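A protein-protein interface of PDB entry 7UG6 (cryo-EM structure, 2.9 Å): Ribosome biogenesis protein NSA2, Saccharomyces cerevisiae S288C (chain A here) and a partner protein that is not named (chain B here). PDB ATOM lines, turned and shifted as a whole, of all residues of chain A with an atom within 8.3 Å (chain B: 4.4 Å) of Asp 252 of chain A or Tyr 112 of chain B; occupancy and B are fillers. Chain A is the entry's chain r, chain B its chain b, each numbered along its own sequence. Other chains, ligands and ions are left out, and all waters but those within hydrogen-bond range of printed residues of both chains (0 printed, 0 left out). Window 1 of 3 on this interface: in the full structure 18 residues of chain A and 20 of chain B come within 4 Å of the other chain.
Among the printed residues, merely in contact across the chains: His 154 of chain A with Leu 115 of chain B, Asp 250 of chain A with Leu 128 of chain B, Asp 252 of chain A with Ala 131 of chain B, Gly 253 of chain A with Tyr 112 of chain B and Gly 253 of chain A with Leu 115 of chain B.
ND1 of His 154 of chain A sits close to O of Pro 249 of chain A (3.2 Å). ND2 of Asn 247 of chain A sits at hydrogen-bond distance from OD2 of Asp 252 of chain A (2.8 Å). N of Asp 250 of chain A sits close to ND1 of His 154 of chain A (3.4 Å).
The side-chain hydroxyl (OH) of Tyr 112 of chain B is in hydrogen-bond range of the backbone carbonyl oxygen (O) of Asp 252 of chain A (3.2 Å).
Of the 13 printed residues of chain B, 4 touch a printed residue of chain A. Hydrophobic or aromatic side chains of chain B that line the printed part of chain A: Tyr 112, Leu 115, Leu 128 and Ala 131. Hydrophobic or aromatic side chains of chain A that line the printed part of chain B: His 154.
Glu 248 of chain A touches none of the printed residues of chain B. Asp 252 of chain A touches two residues of chain B. Of chain A, only Asp 252 and Gly 253 come within 4 Å of Tyr 112 of chain B. Val 113 of chain B touches none of the printed residues of chain A. Of the printed residues of chain A, Leu 115 of chain B touches His 154 (3.6 Å) and Gly 253 (3.6 Å). Of the printed residues of chain A, Leu 128 of chain B touches Asp 250 (3.8 Å). Printed residues of chain A within 4 Å of Ala 131 of chain B: Asp 252. The nearest printed residue of chain B that does not touch Asp 252 of chain A is Leu 128 of chain B (4.6 Å). The nearest printed residue of chain A that does not touch Leu 115 of chain B is Asp 252 of chain A (5.6 Å).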
ATOM      1  N   HIS A 154      10.159 -22.361 -18.864  1.00  0.00           N
ATOM      2  CA  HIS A 154      10.815 -21.223 -18.239  1.00  0.00           C
ATOM      3  C   HIS A 154      11.588 -20.407 -19.261  1.00  0.00           C
ATOM      4  O   HIS A 154      12.123 -20.937 -20.233  1.00  0.00           O
ATOM      5  CB  HIS A 154      11.751 -21.693 -17.137  1.00  0.00           C
ATOM      6  CG  HIS A 154      11.062 -21.951 -15.838  1.00  0.00           C
ATOM      7  ND1 HIS A 154      10.458 -23.149 -15.543  1.00  0.00           N
ATOM      8  CD2 HIS A 154      10.890 -21.166 -14.753  1.00  0.00           C
ATOM      9  CE1 HIS A 154       9.934 -23.089 -14.334  1.00  0.00           C
ATOM     10  NE2 HIS A 154      10.184 -21.897 -13.833  1.00  0.00           N
ATOM     11  N   GLN A 179      13.029 -16.460 -15.311  1.00  0.00           N
ATOM     12  CA  GLN A 179      14.148 -16.808 -14.452  1.00  0.00           C
ATOM     13  C   GLN A 179      15.249 -15.776 -14.605  1.00  0.00           C
ATOM     14  O   GLN A 179      15.605 -15.411 -15.725  1.00  0.00           O
ATOM     15  CB  GLN A 179      14.683 -18.193 -14.798  1.00  0.00           C
ATOM     16  CG  GLN A 179      13.818 -19.324 -14.317  1.00  0.00           C
ATOM     17  CD  GLN A 179      13.660 -19.320 -12.819  1.00  0.00           C
ATOM     18  OE1 GLN A 179      12.741 -18.712 -12.284  1.00  0.00           O
ATOM     19  NE2 GLN A 179      14.567 -19.993 -12.127  1.00  0.00           N
ATOM     20  N   THR A 246      21.231 -28.246 -17.383  1.00  0.00           N
ATOM     21  CA  THR A 246      21.275 -29.694 -17.296  1.00  0.00           C
ATOM     22  C   THR A 246      19.993 -30.330 -16.793  1.00  0.00           C
ATOM     23  O   THR A 246      19.920 -31.557 -16.742  1.00  0.00           O
ATOM     24  CB  THR A 246      22.420 -30.126 -16.387  1.00  0.00           C
ATOM     25  OG1 THR A 246      22.424 -29.305 -15.220  1.00  0.00           O
ATOM     26  CG2 THR A 246      23.727 -29.977 -17.100  1.00  0.00           C
ATOM     27  N   ASN A 247      18.992 -29.556 -16.425  1.00  0.00           N
ATOM     28  CA  ASN A 247      17.745 -30.124 -15.953  1.00  0.00           C
ATOM     29  C   ASN A 247      16.589 -29.544 -16.747  1.00  0.00           C
ATOM     30  O   ASN A 247      16.780 -28.787 -17.698  1.00  0.00           O
ATOM     31  CB  ASN A 247      17.564 -29.875 -14.461  1.00  0.00           C
ATOM     32  CG  ASN A 247      17.142 -28.469 -14.151  1.00  0.00           C
ATOM     33  OD1 ASN A 247      17.657 -27.520 -14.717  1.00  0.00           O
ATOM     34  ND2 ASN A 247      16.207 -28.326 -13.237  1.00  0.00           N
ATOM     35  N   GLU A 248      15.375 -29.914 -16.351  1.00  0.00           N
ATOM     36  CA  GLU A 248      14.153 -29.418 -16.972  1.00  0.00           C
ATOM     37  C   GLU A 248      13.505 -28.463 -15.990  1.00  0.00           C
ATOM     38  O   GLU A 248      12.719 -28.889 -15.139  1.00  0.00           O
ATOM     39  CB  GLU A 248      13.209 -30.567 -17.319  1.00  0.00           C
ATOM     40  CG  GLU A 248      13.638 -31.384 -18.527  1.00  0.00           C
ATOM     41  CD  GLU A 248      13.026 -30.887 -19.820  1.00  0.00           C
ATOM     42  OE1 GLU A 248      12.060 -30.097 -19.754  1.00  0.00           O
ATOM     43  OE2 GLU A 248      13.509 -31.287 -20.901  1.00  0.00           O
ATOM     44  N   PRO A 249      13.806 -27.167 -16.061  1.00  0.00           N
ATOM     45  CA  PRO A 249      13.344 -26.246 -15.015  1.00  0.00           C
ATOM     46  C   PRO A 249      11.846 -26.124 -14.908  1.00  0.00           C
ATOM     47  O   PRO A 249      11.351 -25.679 -13.869  1.00  0.00           O
ATOM     48  CB  PRO A 249      13.979 -24.914 -15.423  1.00  0.00           C
ATOM     49  CG  PRO A 249      14.397 -25.085 -16.797  1.00  0.00           C
ATOM     50  CD  PRO A 249      14.740 -26.510 -16.974  1.00  0.00           C
ATOM     51  N   ASP A 250      11.103 -26.486 -15.950  1.00  0.00           N
ATOM     52  CA  ASP A 250       9.653 -26.425 -15.865  1.00  0.00           C
ATOM     53  C   ASP A 250       9.111 -27.365 -14.805  1.00  0.00           C
ATOM     54  O   ASP A 250       8.089 -27.070 -14.180  1.00  0.00           O
ATOM     55  CB  ASP A 250       9.038 -26.732 -17.227  1.00  0.00           C
ATOM     56  CG  ASP A 250       9.359 -28.136 -17.720  1.00  0.00           C
ATOM     57  OD1 ASP A 250      10.098 -28.877 -17.042  1.00  0.00           O
ATOM     58  OD2 ASP A 250       8.845 -28.519 -18.788  1.00  0.00           O
ATOM     59  N   ARG A 251       9.776 -28.497 -14.587  1.00  0.00           N
ATOM     60  CA  ARG A 251       9.313 -29.507 -13.650  1.00  0.00           C
ATOM     61  C   ARG A 251      10.262 -29.684 -12.479  1.00  0.00           C
ATOM     62  O   ARG A 251      10.181 -30.682 -11.763  1.00  0.00           O
ATOM     63  CB  ARG A 251       9.085 -30.833 -14.372  1.00  0.00           C
ATOM     64  CG  ARG A 251      10.274 -31.388 -15.078  1.00  0.00           C
ATOM     65  CD  ARG A 251       9.858 -32.534 -15.969  1.00  0.00           C
ATOM     66  NE  ARG A 251      10.952 -33.469 -16.189  1.00  0.00           N
ATOM     67  CZ  ARG A 251      11.166 -34.133 -17.319  1.00  0.00           C
ATOM     68  NH1 ARG A 251      10.359 -33.979 -18.358  1.00  0.00           N
ATOM     69  NH2 ARG A 251      12.198 -34.956 -17.405  1.00  0.00           N
ATOM     70  N   ASP A 252      11.160 -28.735 -12.269  1.00  0.00           N
ATOM     71  CA  ASP A 252      11.991 -28.699 -11.080  1.00  0.00           C
ATOM     72  C   ASP A 252      11.867 -27.405 -10.307  1.00  0.00           C
ATOM     73  O   ASP A 252      12.205 -27.387  -9.121  1.00  0.00           O
ATOM     74  CB  ASP A 252      13.468 -28.899 -11.440  1.00  0.00           C
ATOM     75  CG  ASP A 252      13.778 -30.298 -11.921  1.00  0.00           C
ATOM     76  OD1 ASP A 252      12.862 -31.131 -11.998  1.00  0.00           O
ATOM     77  OD2 ASP A 252      14.948 -30.563 -12.250  1.00  0.00           O
ATOM     78  N   GLY A 253      11.388 -26.344 -10.917  1.00  0.00           N
ATOM     79  CA  GLY A 253      11.366 -25.036 -10.297  1.00  0.00           C
ATOM     80  C   GLY A 253      12.561 -24.195 -10.627  1.00  0.00           C
ATOM     81  O   GLY A 253      12.421 -23.098 -11.157  1.00  0.00           O
ATOM     82  N   CYS A 254      13.747 -24.697 -10.331  1.00  0.00           N
ATOM     83  CA  CYS A 254      14.990 -23.979 -10.538  1.00  0.00           C
ATOM     84  C   CYS A 254      15.611 -24.354 -11.877  1.00  0.00           C
ATOM     85  O   CYS A 254      15.289 -25.376 -12.476  1.00  0.00           O
ATOM     86  CB  CYS A 254      15.959 -24.296  -9.410  1.00  0.00           C
ATOM     87  SG  CYS A 254      16.095 -26.069  -9.133  1.00  0.00           S
ATOM     88  N   VAL A 255      16.531 -23.510 -12.333  1.00  0.00           N
ATOM     89  CA  VAL A 255      17.319 -23.761 -13.532  1.00  0.00           C
ATOM     90  C   VAL A 255      18.691 -24.215 -13.083  1.00  0.00           C
ATOM     91  O   VAL A 255      19.410 -23.466 -12.418  1.00  0.00           O
ATOM     92  CB  VAL A 255      17.434 -22.514 -14.414  1.00  0.00           C
ATOM     93  CG1 VAL A 255      18.357 -22.778 -15.568  1.00  0.00           C
ATOM     94  CG2 VAL A 255      16.086 -22.103 -14.908  1.00  0.00           C
ATOM     95  N   ASN A 256      19.058 -25.434 -13.442  1.00  0.00           N
ATOM     96  CA  ASN A 256      20.333 -26.008 -13.049  1.00  0.00           C
ATOM     97  C   ASN A 256      21.224 -26.147 -14.270  1.00  0.00           C
ATOM     98  O   ASN A 256      20.896 -26.885 -15.199  1.00  0.00           O
ATOM     99  CB  ASN A 256      20.120 -27.366 -12.397  1.00  0.00           C
ATOM    100  CG  ASN A 256      19.724 -27.248 -10.964  1.00  0.00           C
ATOM    101  OD1 ASN A 256      18.808 -27.912 -10.506  1.00  0.00           O
ATOM    102  ND2 ASN A 256      20.413 -26.396 -10.240  1.00  0.00           N
ATOM    103  N   VAL B 108       9.412 -20.922  -0.246  1.00  0.00           N
ATOM    104  CA  VAL B 108       9.337 -22.087  -1.122  1.00  0.00           C
ATOM    105  C   VAL B 108       7.889 -22.400  -1.454  1.00  0.00           C
ATOM    106  O   VAL B 108       7.543 -22.689  -2.606  1.00  0.00           O
ATOM    107  CB  VAL B 108      10.041 -23.290  -0.475  1.00  0.00           C
ATOM    108  CG1 VAL B 108       9.663 -24.558  -1.182  1.00  0.00           C
ATOM    109  CG2 VAL B 108      11.530 -23.104  -0.516  1.00  0.00           C
ATOM    110  N   ALA B 109       7.017 -22.330  -0.447  1.00  0.00           N
ATOM    111  CA  ALA B 109       5.605 -22.580  -0.686  1.00  0.00           C
ATOM    112  C   ALA B 109       5.041 -21.593  -1.689  1.00  0.00           C
ATOM    113  O   ALA B 109       4.324 -21.982  -2.611  1.00  0.00           O
ATOM    114  CB  ALA B 109       4.829 -22.508   0.622  1.00  0.00           C
ATOM    115  N   ARG B 110       5.378 -20.314  -1.546  1.00  0.00           N
ATOM    116  CA  ARG B 110       4.855 -19.316  -2.469  1.00  0.00           C
ATOM    117  C   ARG B 110       5.364 -19.544  -3.886  1.00  0.00           C
ATOM    118  O   ARG B 110       4.588 -19.514  -4.850  1.00  0.00           O
ATOM    119  CB  ARG B 110       5.222 -17.927  -1.982  1.00  0.00           C
ATOM    120  CG  ARG B 110       4.177 -17.374  -1.085  1.00  0.00           C
ATOM    121  CD  ARG B 110       4.343 -15.912  -0.868  1.00  0.00           C
ATOM    122  NE  ARG B 110       5.700 -15.560  -0.485  1.00  0.00           N
ATOM    123  CZ  ARG B 110       6.076 -15.366   0.768  1.00  0.00           C
ATOM    124  NH1 ARG B 110       5.191 -15.503   1.742  1.00  0.00           N
ATOM    125  NH2 ARG B 110       7.330 -15.043   1.048  1.00  0.00           N
ATOM    126  N   ASP B 111       6.665 -19.795  -4.029  1.00  0.00           N
ATOM    127  CA  ASP B 111       7.235 -20.002  -5.356  1.00  0.00           C
ATOM    128  C   ASP B 111       6.584 -21.178  -6.057  1.00  0.00           C
ATOM    129  O   ASP B 111       6.220 -21.091  -7.233  1.00  0.00           O
ATOM    130  CB  ASP B 111       8.738 -20.231  -5.258  1.00  0.00           C
ATOM    131  CG  ASP B 111       9.468 -19.035  -4.734  1.00  0.00           C
ATOM    132  OD1 ASP B 111       8.815 -17.995  -4.526  1.00  0.00           O
ATOM    133  OD2 ASP B 111      10.693 -19.132  -4.528  1.00  0.00           O
ATOM    134  N   TYR B 112       6.413 -22.287  -5.350  1.00  0.00           N
ATOM    135  CA  TYR B 112       5.930 -23.476  -6.028  1.00  0.00           C
ATOM    136  C   TYR B 112       4.421 -23.516  -6.159  1.00  0.00           C
ATOM    137  O   TYR B 112       3.910 -24.266  -6.989  1.00  0.00           O
ATOM    138  CB  TYR B 112       6.444 -24.704  -5.314  1.00  0.00           C
ATOM    139  CG  TYR B 112       7.886 -24.930  -5.642  1.00  0.00           C
ATOM    140  CD1 TYR B 112       8.876 -24.261  -4.959  1.00  0.00           C
ATOM    141  CD2 TYR B 112       8.253 -25.769  -6.663  1.00  0.00           C
ATOM    142  CE1 TYR B 112      10.184 -24.447  -5.266  1.00  0.00           C
ATOM    143  CE2 TYR B 112       9.559 -25.957  -6.973  1.00  0.00           C
ATOM    144  CZ  TYR B 112      10.521 -25.295  -6.271  1.00  0.00           C
ATOM    145  OH  TYR B 112      11.840 -25.482  -6.580  1.00  0.00           O
ATOM    146  N   VAL B 113       3.695 -22.726  -5.379  1.00  0.00           N
ATOM    147  CA  VAL B 113       2.298 -22.482  -5.701  1.00  0.00           C
ATOM    148  C   VAL B 113       2.182 -21.663  -6.974  1.00  0.00           C
ATOM    149  O   VAL B 113       1.311 -21.920  -7.810  1.00  0.00           O
ATOM    150  CB  VAL B 113       1.599 -21.819  -4.508  1.00  0.00           C
ATOM    151  CG1 VAL B 113       0.250 -21.380  -4.877  1.00  0.00           C
ATOM    152  CG2 VAL B 113       1.450 -22.832  -3.415  1.00  0.00           C
ATOM    153  N   ARG B 114       3.064 -20.677  -7.163  1.00  0.00           N
ATOM    154  CA  ARG B 114       3.032 -19.936  -8.420  1.00  0.00           C
ATOM    155  C   ARG B 114       3.412 -20.802  -9.609  1.00  0.00           C
ATOM    156  O   ARG B 114       2.838 -20.652 -10.686  1.00  0.00           O
ATOM    157  CB  ARG B 114       3.934 -18.710  -8.366  1.00  0.00           C
ATOM    158  CG  ARG B 114       3.199 -17.472  -7.949  1.00  0.00           C
ATOM    159  CD  ARG B 114       4.050 -16.245  -8.104  1.00  0.00           C
ATOM    160  NE  ARG B 114       5.076 -16.162  -7.077  1.00  0.00           N
ATOM    161  CZ  ARG B 114       6.071 -15.284  -7.101  1.00  0.00           C
ATOM    162  NH1 ARG B 114       6.166 -14.418  -8.100  1.00  0.00           N
ATOM    163  NH2 ARG B 114       6.972 -15.273  -6.129  1.00  0.00           N
ATOM    164  N   LEU B 115       4.384 -21.687  -9.453  1.00  0.00           N
ATOM    165  CA  LEU B 115       4.767 -22.529 -10.578  1.00  0.00           C
ATOM    166  C   LEU B 115       3.705 -23.562 -10.919  1.00  0.00           C
ATOM    167  O   LEU B 115       3.491 -23.862 -12.095  1.00  0.00           O
ATOM    168  CB  LEU B 115       6.090 -23.224 -10.280  1.00  0.00           C
ATOM    169  CG  LEU B 115       7.258 -22.265 -10.149  1.00  0.00           C
ATOM    170  CD1 LEU B 115       8.449 -23.025  -9.691  1.00  0.00           C
ATOM    171  CD2 LEU B 115       7.536 -21.599 -11.462  1.00  0.00           C
ATOM    172  N   LEU B 116       3.044 -24.120  -9.907  1.00  0.00           N
ATOM    173  CA  LEU B 116       1.966 -25.071 -10.133  1.00  0.00           C
ATOM    174  C   LEU B 116       0.790 -24.430 -10.832  1.00  0.00           C
ATOM    175  O   LEU B 116       0.033 -25.121 -11.517  1.00  0.00           O
ATOM    176  CB  LEU B 116       1.515 -25.656  -8.804  1.00  0.00           C
ATOM    177  CG  LEU B 116       2.363 -26.806  -8.292  1.00  0.00           C
ATOM    178  CD1 LEU B 116       2.127 -27.021  -6.826  1.00  0.00           C
ATOM    179  CD2 LEU B 116       2.015 -28.036  -9.058  1.00  0.00           C
ATOM    180  N   LEU B 128       6.552 -30.749  -9.536  1.00  0.00           N
ATOM    181  CA  LEU B 128       6.638 -29.480  -8.827  1.00  0.00           C
ATOM    182  C   LEU B 128       6.281 -29.639  -7.355  1.00  0.00           C
ATOM    183  O   LEU B 128       6.941 -29.057  -6.488  1.00  0.00           O
ATOM    184  CB  LEU B 128       5.740 -28.450  -9.492  1.00  0.00           C
ATOM    185  CG  LEU B 128       6.270 -27.867 -10.789  1.00  0.00           C
ATOM    186  CD1 LEU B 128       5.145 -27.205 -11.517  1.00  0.00           C
ATOM    187  CD2 LEU B 128       7.344 -26.876 -10.489  1.00  0.00           C
ATOM    188  N   ALA B 131       9.151 -31.410  -5.748  1.00  0.00           N
ATOM    189  CA  ALA B 131      10.253 -30.473  -5.619  1.00  0.00           C
ATOM    190  C   ALA B 131      10.051 -29.551  -4.429  1.00  0.00           C
ATOM    191  O   ALA B 131      10.973 -29.338  -3.640  1.00  0.00           O
ATOM    192  CB  ALA B 131      10.400 -29.671  -6.906  1.00  0.00           C
ATOM    193  N   ALA B 132       8.848 -29.001  -4.277  1.00  0.00           N
ATOM    194  CA  ALA B 132       8.587 -28.096  -3.164  1.00  0.00           C
ATOM    195  C   ALA B 132       8.729 -28.816  -1.837  1.00  0.00           C
ATOM    196  O   ALA B 132       9.333 -28.299  -0.890  1.00  0.00           O
ATOM    197  CB  ALA B 132       7.192 -27.503  -3.287  1.00  0.00           C
ATOM    198  N   ARG B 135      12.315 -29.431  -1.071  1.00  0.00           N
ATOM    199  CA  ARG B 135      12.993 -28.214  -0.651  1.00  0.00           C
ATOM    200  C   ARG B 135      12.696 -27.901   0.804  1.00  0.00           C
ATOM    201  O   ARG B 135      13.597 -27.527   1.561  1.00  0.00           O
ATOM    202  CB  ARG B 135      12.590 -27.056  -1.553  1.00  0.00           C
ATOM    203  CG  ARG B 135      13.123 -27.183  -2.959  1.00  0.00           C
ATOM    204  CD  ARG B 135      13.199 -25.852  -3.654  1.00  0.00           C
ATOM    205  NE  ARG B 135      14.079 -24.936  -2.950  1.00  0.00           N
ATOM    206  CZ  ARG B 135      14.690 -23.910  -3.525  1.00  0.00           C
ATOM    207  NH1 ARG B 135      14.512 -23.675  -4.815  1.00  0.00           N
ATOM    208  NH2 ARG B 135      15.478 -23.121  -2.813  1.00  0.00           N
